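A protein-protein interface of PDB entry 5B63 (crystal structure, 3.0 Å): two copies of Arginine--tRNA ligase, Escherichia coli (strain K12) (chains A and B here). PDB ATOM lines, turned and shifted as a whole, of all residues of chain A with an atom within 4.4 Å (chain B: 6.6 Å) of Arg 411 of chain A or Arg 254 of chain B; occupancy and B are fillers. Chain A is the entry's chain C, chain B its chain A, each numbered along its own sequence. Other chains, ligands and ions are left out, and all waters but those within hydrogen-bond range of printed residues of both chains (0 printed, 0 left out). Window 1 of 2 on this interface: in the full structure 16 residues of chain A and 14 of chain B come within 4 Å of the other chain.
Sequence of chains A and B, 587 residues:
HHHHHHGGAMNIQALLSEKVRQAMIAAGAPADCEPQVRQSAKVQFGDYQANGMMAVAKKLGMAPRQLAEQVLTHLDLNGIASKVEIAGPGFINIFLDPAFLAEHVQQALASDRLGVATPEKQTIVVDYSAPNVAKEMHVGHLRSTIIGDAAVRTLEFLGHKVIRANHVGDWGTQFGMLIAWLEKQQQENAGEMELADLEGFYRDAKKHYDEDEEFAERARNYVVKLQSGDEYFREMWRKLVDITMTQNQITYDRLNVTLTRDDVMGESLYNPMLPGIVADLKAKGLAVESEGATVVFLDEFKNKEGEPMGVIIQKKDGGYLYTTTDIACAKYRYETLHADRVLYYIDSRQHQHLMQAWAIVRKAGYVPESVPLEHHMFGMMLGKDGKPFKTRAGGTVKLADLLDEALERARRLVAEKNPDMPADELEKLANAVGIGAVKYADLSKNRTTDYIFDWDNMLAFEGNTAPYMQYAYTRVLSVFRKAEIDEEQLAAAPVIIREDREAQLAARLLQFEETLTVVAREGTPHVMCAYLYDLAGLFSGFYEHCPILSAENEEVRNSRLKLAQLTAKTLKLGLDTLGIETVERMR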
ATOM      1  N   LEU A 407      32.086  14.519  27.558  1.00  0.00           N
ATOM      2  CA  LEU A 407      30.638  14.435  27.651  1.00  0.00           C
ATOM      3  C   LEU A 407      30.206  13.216  28.456  1.00  0.00           C
ATOM      4  O   LEU A 407      29.288  13.296  29.270  1.00  0.00           O
ATOM      5  CB  LEU A 407      30.018  14.408  26.253  1.00  0.00           C
ATOM      6  CG  LEU A 407      29.502  15.757  25.762  1.00  0.00           C
ATOM      7  CD1 LEU A 407      29.006  15.667  24.333  1.00  0.00           C
ATOM      8  CD2 LEU A 407      28.394  16.203  26.682  1.00  0.00           C
ATOM      9  N   GLU A 408      30.878  12.090  28.238  1.00  0.00           N
ATOM     10  CA  GLU A 408      30.524  10.856  28.930  1.00  0.00           C
ATOM     11  C   GLU A 408      30.841  10.920  30.420  1.00  0.00           C
ATOM     12  O   GLU A 408      30.017  10.542  31.252  1.00  0.00           O
ATOM     13  CB  GLU A 408      31.224   9.652  28.292  1.00  0.00           C
ATOM     14  CG  GLU A 408      30.902   8.314  28.954  1.00  0.00           C
ATOM     15  CD  GLU A 408      29.485   7.829  28.686  1.00  0.00           C
ATOM     16  OE1 GLU A 408      28.746   8.488  27.923  1.00  0.00           O
ATOM     17  OE2 GLU A 408      29.111   6.775  29.242  1.00  0.00           O
ATOM     18  N   ARG A 409      32.033  11.403  30.754  1.00  0.00           N
ATOM     19  CA  ARG A 409      32.446  11.487  32.149  1.00  0.00           C
ATOM     20  C   ARG A 409      31.633  12.549  32.886  1.00  0.00           C
ATOM     21  O   ARG A 409      31.521  12.523  34.112  1.00  0.00           O
ATOM     22  CB  ARG A 409      33.945  11.778  32.261  1.00  0.00           C
ATOM     23  CG  ARG A 409      34.533  11.438  33.624  1.00  0.00           C
ATOM     24  CD  ARG A 409      35.960  11.943  33.763  1.00  0.00           C
ATOM     25  NE  ARG A 409      36.948  10.870  33.723  1.00  0.00           N
ATOM     26  CZ  ARG A 409      37.526  10.429  32.610  1.00  0.00           C
ATOM     27  NH1 ARG A 409      37.210  10.967  31.440  1.00  0.00           N
ATOM     28  NH2 ARG A 409      38.419   9.450  32.668  1.00  0.00           N
ATOM     29  N   ALA A 410      31.063  13.480  32.129  1.00  0.00           N
ATOM     30  CA  ALA A 410      30.170  14.483  32.695  1.00  0.00           C
ATOM     31  C   ALA A 410      28.826  13.835  32.992  1.00  0.00           C
ATOM     32  O   ALA A 410      28.190  14.134  34.005  1.00  0.00           O
ATOM     33  CB  ALA A 410      29.992  15.639  31.733  1.00  0.00           C
ATOM     34  N   ARG A 411      28.403  12.947  32.095  1.00  0.00           N
ATOM     35  CA  ARG A 411      27.144  12.232  32.253  1.00  0.00           C
ATOM     36  C   ARG A 411      27.160  11.414  33.533  1.00  0.00           C
ATOM     37  O   ARG A 411      26.204  11.436  34.307  1.00  0.00           O
ATOM     38  CB  ARG A 411      26.884  11.321  31.053  1.00  0.00           C
ATOM     39  CG  ARG A 411      26.483  12.046  29.786  1.00  0.00           C
ATOM     40  CD  ARG A 411      26.283  11.064  28.647  1.00  0.00           C
ATOM     41  NE  ARG A 411      25.920  11.730  27.402  1.00  0.00           N
ATOM     42  CZ  ARG A 411      26.712  11.809  26.338  1.00  0.00           C
ATOM     43  NH1 ARG A 411      27.916  11.252  26.363  1.00  0.00           N
ATOM     44  NH2 ARG A 411      26.297  12.437  25.248  1.00  0.00           N
ATOM     45  N   ARG A 412      28.259  10.701  33.752  1.00  0.00           N
ATOM     46  CA  ARG A 412      28.429   9.919  34.965  1.00  0.00           C
ATOM     47  C   ARG A 412      28.458  10.831  36.182  1.00  0.00           C
ATOM     48  O   ARG A 412      27.929  10.489  37.240  1.00  0.00           O
ATOM     49  CB  ARG A 412      29.729   9.124  34.904  1.00  0.00           C
ATOM     50  CG  ARG A 412      29.929   8.358  33.617  1.00  0.00           C
ATOM     51  CD  ARG A 412      31.271   7.658  33.636  1.00  0.00           C
ATOM     52  NE  ARG A 412      31.705   7.242  32.308  1.00  0.00           N
ATOM     53  CZ  ARG A 412      32.005   5.991  31.980  1.00  0.00           C
ATOM     54  NH1 ARG A 412      31.918   5.030  32.887  1.00  0.00           N
ATOM     55  NH2 ARG A 412      32.396   5.702  30.748  1.00  0.00           N
ATOM     56  N   LEU A 413      29.079  11.995  36.021  1.00  0.00           N
ATOM     57  CA  LEU A 413      29.231  12.950  37.111  1.00  0.00           C
ATOM     58  C   LEU A 413      27.887  13.513  37.565  1.00  0.00           C
ATOM     59  O   LEU A 413      27.648  13.678  38.761  1.00  0.00           O
ATOM     60  CB  LEU A 413      30.164  14.090  36.692  1.00  0.00           C
ATOM     61  CG  LEU A 413      30.402  15.211  37.705  1.00  0.00           C
ATOM     62  CD1 LEU A 413      31.257  14.707  38.851  1.00  0.00           C
ATOM     63  CD2 LEU A 413      31.047  16.419  37.041  1.00  0.00           C
ATOM     64  N   VAL A 414      27.016  13.810  36.606  1.00  0.00           N
ATOM     65  CA  VAL A 414      25.710  14.389  36.908  1.00  0.00           C
ATOM     66  C   VAL A 414      24.712  13.324  37.346  1.00  0.00           C
ATOM     67  O   VAL A 414      24.029  13.479  38.359  1.00  0.00           O
ATOM     68  CB  VAL A 414      25.136  15.156  35.702  1.00  0.00           C
ATOM     69  CG1 VAL A 414      23.743  15.680  36.018  1.00  0.00           C
ATOM     70  CG2 VAL A 414      26.060  16.297  35.317  1.00  0.00           C
ATOM     71  N   ALA A 415      24.634  12.238  36.584  1.00  0.00           N
ATOM     72  CA  ALA A 415      23.737  11.137  36.917  1.00  0.00           C
ATOM     73  C   ALA A 415      24.281  10.334  38.095  1.00  0.00           C
ATOM     74  O   ALA A 415      24.481   9.124  37.999  1.00  0.00           O
ATOM     75  CB  ALA A 415      23.525  10.241  35.710  1.00  0.00           C
ATOM     76  N   GLU A 427      21.620  15.842  29.285  1.00  0.00           N
ATOM     77  CA  GLU A 427      22.476  16.123  28.142  1.00  0.00           C
ATOM     78  C   GLU A 427      22.684  17.623  28.035  1.00  0.00           C
ATOM     79  O   GLU A 427      23.693  18.086  27.509  1.00  0.00           O
ATOM     80  CB  GLU A 427      21.856  15.583  26.856  1.00  0.00           C
ATOM     81  CG  GLU A 427      21.968  14.081  26.714  1.00  0.00           C
ATOM     82  CD  GLU A 427      23.409  13.620  26.626  1.00  0.00           C
ATOM     83  OE1 GLU A 427      24.118  14.061  25.698  1.00  0.00           O
ATOM     84  OE2 GLU A 427      23.833  12.824  27.490  1.00  0.00           O
ATOM     85  N   ALA A 430      25.342  17.866  31.132  1.00  0.00           N
ATOM     86  CA  ALA A 430      26.591  17.202  30.765  1.00  0.00           C
ATOM     87  C   ALA A 430      27.322  17.894  29.621  1.00  0.00           C
ATOM     88  O   ALA A 430      28.548  17.839  29.537  1.00  0.00           O
ATOM     89  CB  ALA A 430      26.335  15.746  30.421  1.00  0.00           C
ATOM     90  N   GLN B 249      21.708   3.135  33.012  1.00  0.00           N
ATOM     91  CA  GLN B 249      20.557   4.025  32.990  1.00  0.00           C
ATOM     92  C   GLN B 249      20.904   5.263  32.180  1.00  0.00           C
ATOM     93  O   GLN B 249      20.040   5.870  31.549  1.00  0.00           O
ATOM     94  CB  GLN B 249      20.138   4.422  34.402  1.00  0.00           C
ATOM     95  CG  GLN B 249      18.836   5.203  34.443  1.00  0.00           C
ATOM     96  CD  GLN B 249      17.660   4.400  33.918  1.00  0.00           C
ATOM     97  OE1 GLN B 249      17.567   3.193  34.142  1.00  0.00           O
ATOM     98  NE2 GLN B 249      16.763   5.066  33.204  1.00  0.00           N
ATOM     99  N   ILE B 250      22.180   5.631  32.213  1.00  0.00           N
ATOM    100  CA  ILE B 250      22.691   6.716  31.391  1.00  0.00           C
ATOM    101  C   ILE B 250      22.566   6.343  29.924  1.00  0.00           C
ATOM    102  O   ILE B 250      22.099   7.135  29.107  1.00  0.00           O
ATOM    103  CB  ILE B 250      24.172   6.985  31.687  1.00  0.00           C
ATOM    104  CG1 ILE B 250      24.355   7.479  33.121  1.00  0.00           C
ATOM    105  CG2 ILE B 250      24.734   7.996  30.703  1.00  0.00           C
ATOM    106  CD1 ILE B 250      25.803   7.677  33.505  1.00  0.00           C
ATOM    107  N   THR B 251      22.992   5.128  29.600  1.00  0.00           N
ATOM    108  CA  THR B 251      22.932   4.635  28.232  1.00  0.00           C
ATOM    109  C   THR B 251      21.490   4.570  27.750  1.00  0.00           C
ATOM    110  O   THR B 251      21.202   4.858  26.591  1.00  0.00           O
ATOM    111  CB  THR B 251      23.558   3.237  28.110  1.00  0.00           C
ATOM    112  OG1 THR B 251      24.856   3.236  28.716  1.00  0.00           O
ATOM    113  CG2 THR B 251      23.686   2.843  26.648  1.00  0.00           C
ATOM    114  N   TYR B 252      20.588   4.191  28.650  1.00  0.00           N
ATOM    115  CA  TYR B 252      19.166   4.137  28.331  1.00  0.00           C
ATOM    116  C   TYR B 252      18.628   5.532  28.038  1.00  0.00           C
ATOM    117  O   TYR B 252      17.951   5.751  27.033  1.00  0.00           O
ATOM    118  CB  TYR B 252      18.382   3.520  29.490  1.00  0.00           C
ATOM    119  CG  TYR B 252      18.602   2.037  29.679  1.00  0.00           C
ATOM    120  CD1 TYR B 252      18.967   1.228  28.611  1.00  0.00           C
ATOM    121  CD2 TYR B 252      18.443   1.445  30.924  1.00  0.00           C
ATOM    122  CE1 TYR B 252      19.168  -0.131  28.781  1.00  0.00           C
ATOM    123  CE2 TYR B 252      18.641   0.090  31.104  1.00  0.00           C
ATOM    124  CZ  TYR B 252      19.005  -0.693  30.028  1.00  0.00           C
ATOM    125  OH  TYR B 252      19.204  -2.044  30.203  1.00  0.00           O
ATOM    126  N   ASP B 253      18.943   6.465  28.932  1.00  0.00           N
ATOM    127  CA  ASP B 253      18.505   7.851  28.816  1.00  0.00           C
ATOM    128  C   ASP B 253      19.000   8.472  27.519  1.00  0.00           C
ATOM    129  O   ASP B 253      18.313   9.291  26.904  1.00  0.00           O
ATOM    130  CB  ASP B 253      19.011   8.662  30.009  1.00  0.00           C
ATOM    131  CG  ASP B 253      18.300   8.301  31.297  1.00  0.00           C
ATOM    132  OD1 ASP B 253      17.612   7.258  31.324  1.00  0.00           O
ATOM    133  OD2 ASP B 253      18.432   9.056  32.283  1.00  0.00           O
ATOM    134  N   ARG B 254      20.200   8.075  27.112  1.00  0.00           N
ATOM    135  CA  ARG B 254      20.765   8.523  25.851  1.00  0.00           C
ATOM    136  C   ARG B 254      20.014   7.884  24.697  1.00  0.00           C
ATOM    137  O   ARG B 254      19.801   8.499  23.654  1.00  0.00           O
ATOM    138  CB  ARG B 254      22.242   8.144  25.770  1.00  0.00           C
ATOM    139  CG  ARG B 254      23.163   9.111  26.472  1.00  0.00           C
ATOM    140  CD  ARG B 254      24.204   9.644  25.499  1.00  0.00           C
ATOM    141  NE  ARG B 254      25.233   8.654  25.206  1.00  0.00           N
ATOM    142  CZ  ARG B 254      26.112   8.767  24.218  1.00  0.00           C
ATOM    143  NH1 ARG B 254      26.077   9.820  23.415  1.00  0.00           N
ATOM    144  NH2 ARG B 254      27.021   7.823  24.028  1.00  0.00           N
ATOM    145  N   LEU B 255      19.605   6.639  24.908  1.00  0.00           N
ATOM    146  CA  LEU B 255      19.001   5.831  23.862  1.00  0.00           C
ATOM    147  C   LEU B 255      17.506   6.102  23.770  1.00  0.00           C
ATOM    148  O   LEU B 255      16.832   5.603  22.870  1.00  0.00           O
ATOM    149  CB  LEU B 255      19.246   4.354  24.164  1.00  0.00           C
ATOM    150  CG  LEU B 255      19.523   3.382  23.023  1.00  0.00           C
ATOM    151  CD1 LEU B 255      20.132   4.103  21.845  1.00  0.00           C
ATOM    152  CD2 LEU B 255      20.473   2.325  23.535  1.00  0.00           C
ATOM    153  N   ASN B 256      17.006   6.900  24.709  1.00  0.00           N
ATOM    154  CA  ASN B 256      15.581   7.202  24.829  1.00  0.00           C
ATOM    155  C   ASN B 256      14.737   5.956  25.100  1.00  0.00           C
ATOM    156  O   ASN B 256      13.596   5.846  24.649  1.00  0.00           O
ATOM    157  CB  ASN B 256      15.073   7.968  23.602  1.00  0.00           C
ATOM    158  CG  ASN B 256      13.788   8.728  23.878  1.00  0.00           C
ATOM    159  OD1 ASN B 256      13.446   8.993  25.029  1.00  0.00           O
ATOM    160  ND2 ASN B 256      13.071   9.082  22.820  1.00  0.00           N
ATOM    161  N   VAL B 257      15.315   5.019  25.845  1.00  0.00           N
ATOM    162  CA  VAL B 257      14.614   3.814  26.259  1.00  0.00           C
ATOM    163  C   VAL B 257      13.885   4.071  27.575  1.00  0.00           C
ATOM    164  O   VAL B 257      14.428   4.704  28.474  1.00  0.00           O
ATOM    165  CB  VAL B 257      15.598   2.648  26.426  1.00  0.00           C
ATOM    166  CG1 VAL B 257      14.877   1.394  26.879  1.00  0.00           C
ATOM    167  CG2 VAL B 257      16.324   2.398  25.124  1.00  0.00           C
ATOM    168  N   LEU B 399      28.643  -0.112  23.761  1.00  0.00           N
ATOM    169  CA  LEU B 399      27.451   0.560  23.251  1.00  0.00           C
ATOM    170  C   LEU B 399      27.593   2.079  23.289  1.00  0.00           C
ATOM    171  O   LEU B 399      27.114   2.777  22.397  1.00  0.00           O
ATOM    172  CB  LEU B 399      26.211   0.118  24.033  1.00  0.00           C
ATOM    173  CG  LEU B 399      24.870   0.715  23.597  1.00  0.00           C
ATOM    174  CD1 LEU B 399      24.696   0.583  22.098  1.00  0.00           C
ATOM    175  CD2 LEU B 399      23.728   0.032  24.320  1.00  0.00           C
ATOM    176  N   ALA B 400      28.256   2.583  24.323  1.00  0.00           N
ATOM    177  CA  ALA B 400      28.498   4.015  24.448  1.00  0.00           C
ATOM    178  C   ALA B 400      29.343   4.524  23.284  1.00  0.00           C
ATOM    179  O   ALA B 400      29.059   5.574  22.710  1.00  0.00           O
ATOM    180  CB  ALA B 400      29.174   4.323  25.771  1.00  0.00           C
ATOM    181  N   ASP B 401      30.372   3.759  22.934  1.00  0.00           N
ATOM    182  CA  ASP B 401      31.267   4.117  21.838  1.00  0.00           C
ATOM    183  C   ASP B 401      30.551   4.090  20.492  1.00  0.00           C
ATOM    184  O   ASP B 401      30.948   4.779  19.549  1.00  0.00           O
ATOM    185  CB  ASP B 401      32.466   3.171  21.805  1.00  0.00           C
ATOM    186  CG  ASP B 401      33.378   3.344  23.003  1.00  0.00           C
ATOM    187  OD1 ASP B 401      32.943   3.955  24.001  1.00  0.00           O
ATOM    188  OD2 ASP B 401      34.531   2.869  22.945  1.00  0.00           O
ATOM    189  N   LEU B 402      29.496   3.286  20.409  1.00  0.00           N
ATOM    190  CA  LEU B 402      28.697   3.207  19.196  1.00  0.00           C
ATOM    191  C   LEU B 402      27.808   4.437  19.071  1.00  0.00           C
ATOM    192  O   LEU B 402      27.649   4.994  17.985  1.00  0.00           O
ATOM    193  CB  LEU B 402      27.830   1.950  19.199  1.00  0.00           C
ATOM    194  CG  LEU B 402      27.080   1.690  17.891  1.00  0.00           C
ATOM    195  CD1 LEU B 402      27.950   0.903  16.924  1.00  0.00           C
ATOM    196  CD2 LEU B 402      25.767   0.975  18.145  1.00  0.00           C
ATOM    197  N   LEU B 403      27.227   4.853  20.191  1.00  0.00           N
ATOM    198  CA  LEU B 403      26.347   6.012  20.213  1.00  0.00           C
ATOM    199  C   LEU B 403      27.129   7.290  19.938  1.00  0.00           C
ATOM    200  O   LEU B 403      26.609   8.232  19.337  1.00  0.00           O
ATOM    201  CB  LEU B 403      25.623   6.108  21.559  1.00  0.00           C
ATOM    202  CG  LEU B 403      24.694   4.944  21.910  1.00  0.00           C
ATOM    203  CD1 LEU B 403      24.134   5.105  23.314  1.00  0.00           C
ATOM    204  CD2 LEU B 403      23.573   4.823  20.889  1.00  0.00           C
ATOM    205  N   ASP B 404      28.381   7.309  20.383  1.00  0.00           N
ATOM    206  CA  ASP B 404      29.261   8.447  20.160  1.00  0.00           C
ATOM    207  C   ASP B 404      29.507   8.668  18.674  1.00  0.00           C
ATOM    208  O   ASP B 404      29.460   9.799  18.188  1.00  0.00           O
ATOM    209  CB  ASP B 404      30.585   8.253  20.900  1.00  0.00           C
ATOM    210  CG  ASP B 404      30.452   8.473  22.393  1.00  0.00           C
ATOM    211  OD1 ASP B 404      29.566   9.259  22.792  1.00  0.00           O
ATOM    212  OD2 ASP B 404      31.225   7.866  23.167  1.00  0.00           O
ATOM    213  N   LEU B 407      26.329   9.892  16.856  1.00  0.00           N
ATOM    214  CA  LEU B 407      26.134  11.326  17.004  1.00  0.00           C
ATOM    215  C   LEU B 407      27.099  12.119  16.131  1.00  0.00           C
ATOM    216  O   LEU B 407      26.724  13.133  15.547  1.00  0.00           O
ATOM    217  CB  LEU B 407      26.281  11.731  18.471  1.00  0.00           C
ATOM    218  CG  LEU B 407      25.021  11.514  19.305  1.00  0.00           C
ATOM    219  CD1 LEU B 407      25.283  11.763  20.778  1.00  0.00           C
ATOM    220  CD2 LEU B 407      23.935  12.435  18.792  1.00  0.00           C
ATOM    221  N   ARG B 411      26.239  14.431  12.913  1.00  0.00           N
ATOM    222  CA  ARG B 411      26.663  15.826  12.845  1.00  0.00           C
ATOM    223  C   ARG B 411      27.234  16.144  11.475  1.00  0.00           C
ATOM    224  O   ARG B 411      26.918  17.175  10.884  1.00  0.00           O
ATOM    225  CB  ARG B 411      27.708  16.136  13.919  1.00  0.00           C
ATOM    226  CG  ARG B 411      27.176  16.168  15.332  1.00  0.00           C
ATOM    227  CD  ARG B 411      28.289  16.477  16.315  1.00  0.00           C
ATOM    228  NE  ARG B 411      27.870  16.273  17.697  1.00  0.00           N
ATOM    229  CZ  ARG B 411      28.329  15.297  18.473  1.00  0.00           C
ATOM    230  NH1 ARG B 411      29.231  14.450  18.001  1.00  0.00           N
ATOM    231  NH2 ARG B 411      27.895  15.178  19.720  1.00  0.00           N
ATOM    232  N   ASN B 431      21.008  14.639  17.526  1.00  0.00           N
ATOM    233  CA  ASN B 431      20.550  13.639  18.475  1.00  0.00           C
ATOM    234  C   ASN B 431      19.431  12.817  17.855  1.00  0.00           C
ATOM    235  O   ASN B 431      19.475  11.590  17.847  1.00  0.00           O
ATOM    236  CB  ASN B 431      20.062  14.306  19.755  1.00  0.00           C
ATOM    237  CG  ASN B 431      20.056  13.361  20.934  1.00  0.00           C
ATOM    238  OD1 ASN B 431      20.916  12.490  21.053  1.00  0.00           O
ATOM    239  ND2 ASN B 431      19.080  13.526  21.815  1.00  0.00           N
ATOM    240  N   ILE B 435      20.710   9.103  16.959  1.00  0.00           N
ATOM    241  CA  ILE B 435      20.144   8.139  17.898  1.00  0.00           C
ATOM    242  C   ILE B 435      18.919   7.443  17.304  1.00  0.00           C
ATOM    243  O   ILE B 435      18.671   6.264  17.566  1.00  0.00           O
ATOM    244  CB  ILE B 435      19.805   8.809  19.254  1.00  0.00           C
ATOM    245  CG1 ILE B 435      20.783   8.345  20.332  1.00  0.00           C
ATOM    246  CG2 ILE B 435      18.382   8.510  19.683  1.00  0.00           C
ATOM    247  CD1 ILE B 435      22.221   8.567  19.968  1.00  0.00           C
ATOM    248  N   LYS B 439      18.294   3.219  16.420  1.00  0.00           N
ATOM    249  CA  LYS B 439      17.105   2.469  16.797  1.00  0.00           C
ATOM    250  C   LYS B 439      16.356   2.005  15.552  1.00  0.00           C
ATOM    251  O   LYS B 439      16.232   0.806  15.306  1.00  0.00           O
ATOM    252  CB  LYS B 439      16.207   3.317  17.698  1.00  0.00           C
ATOM    253  CG  LYS B 439      16.929   3.877  18.914  1.00  0.00           C
ATOM    254  CD  LYS B 439      16.091   4.895  19.657  1.00  0.00           C
ATOM    255  CE  LYS B 439      15.043   4.228  20.531  1.00  0.00           C
ATOM    256  NZ  LYS B 439      14.323   5.226  21.368  1.00  0.00           N
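Ile 250 of chain B touches Arg 411 of chain A.
CA of Arg 412 of chain A touches CD1 of Ile 250 of chain B, at 3.7 Å.
Ala 415 of chain A touches Ile 250 of chain B.
Glu 427 of chain A touches Arg 254 of chain B (OE2 to CD, 3.8 Å).
2 positions are printed for both chains.
Arg 411 of chain A touches two residues of chain B.
Of the printed residues of chain B, Ala 415 of chain A touches Ile 250.
Printed residues of chain B within 4 Å of Glu 427 of chain A: Arg 254.
Of the printed residues of chain A, Ile 250 of chain B touches Arg 411 (3.9 Å), Arg 412 (3.7 Å) and Ala 415 (3.9 Å).
Thr 251 of chain B touches none of the printed residues of chain A.
Arg 254 of chain B touches just these residues of chain A: Arg 411 (3.2 Å) and Glu 427 (3.8 Å).
The nearest residue of chain B that does not touch Arg 411 of chain A is Asp 404 of chain B (4.4 Å).
The nearest residue of chain A that does not touch Arg 254 of chain B is Glu 408 of chain A (4.3 Å).
Of the 11 printed residues of chain A, 4 touch a printed residue of chain B.
Hydrophobic or aromatic side chains of chain A that line the printed part of chain B: Ala 415.
Of the 20 printed residues of chain B, 2 touch a printed residue of chain A.
Among the printed residues, 5 pairs touch across the chains.
Among the printed residues, no Asp or Glu carboxylate lies within 4 Å of a Lys or Arg side-chain nitrogen of the other chain.
NH2 of Arg 411 of chain A sits close to NH1 of Arg 254 of chain B, at 3.2 Å.
The guanidinium group of Arg 254 of chain B sits at hydrogen-bond distance from the backbone carbonyl oxygen of Ala 400 of chain B (3.3 Å).
The guanidinium group (NH2) of Arg 254 of chain B lies within salt-bridge range of the side-chain carboxylate (OD1) of Asp 404 of chain B (3.2 Å).
The side-chain carboxylate of Glu 408 of chain A is in salt-bridge range of the guanidinium group of Arg 411 of chain A (3.3 Å).
The guanidinium group (NH2) of Arg 412 of chain A lies within salt-bridge range of the side-chain carboxylate (OE2) of Glu 408 of chain A.
The guanidinium group (NH2) of Arg 411 of chain A is in salt-bridge range of the side-chain carboxylate (OE1) of Glu 427 of chain A.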
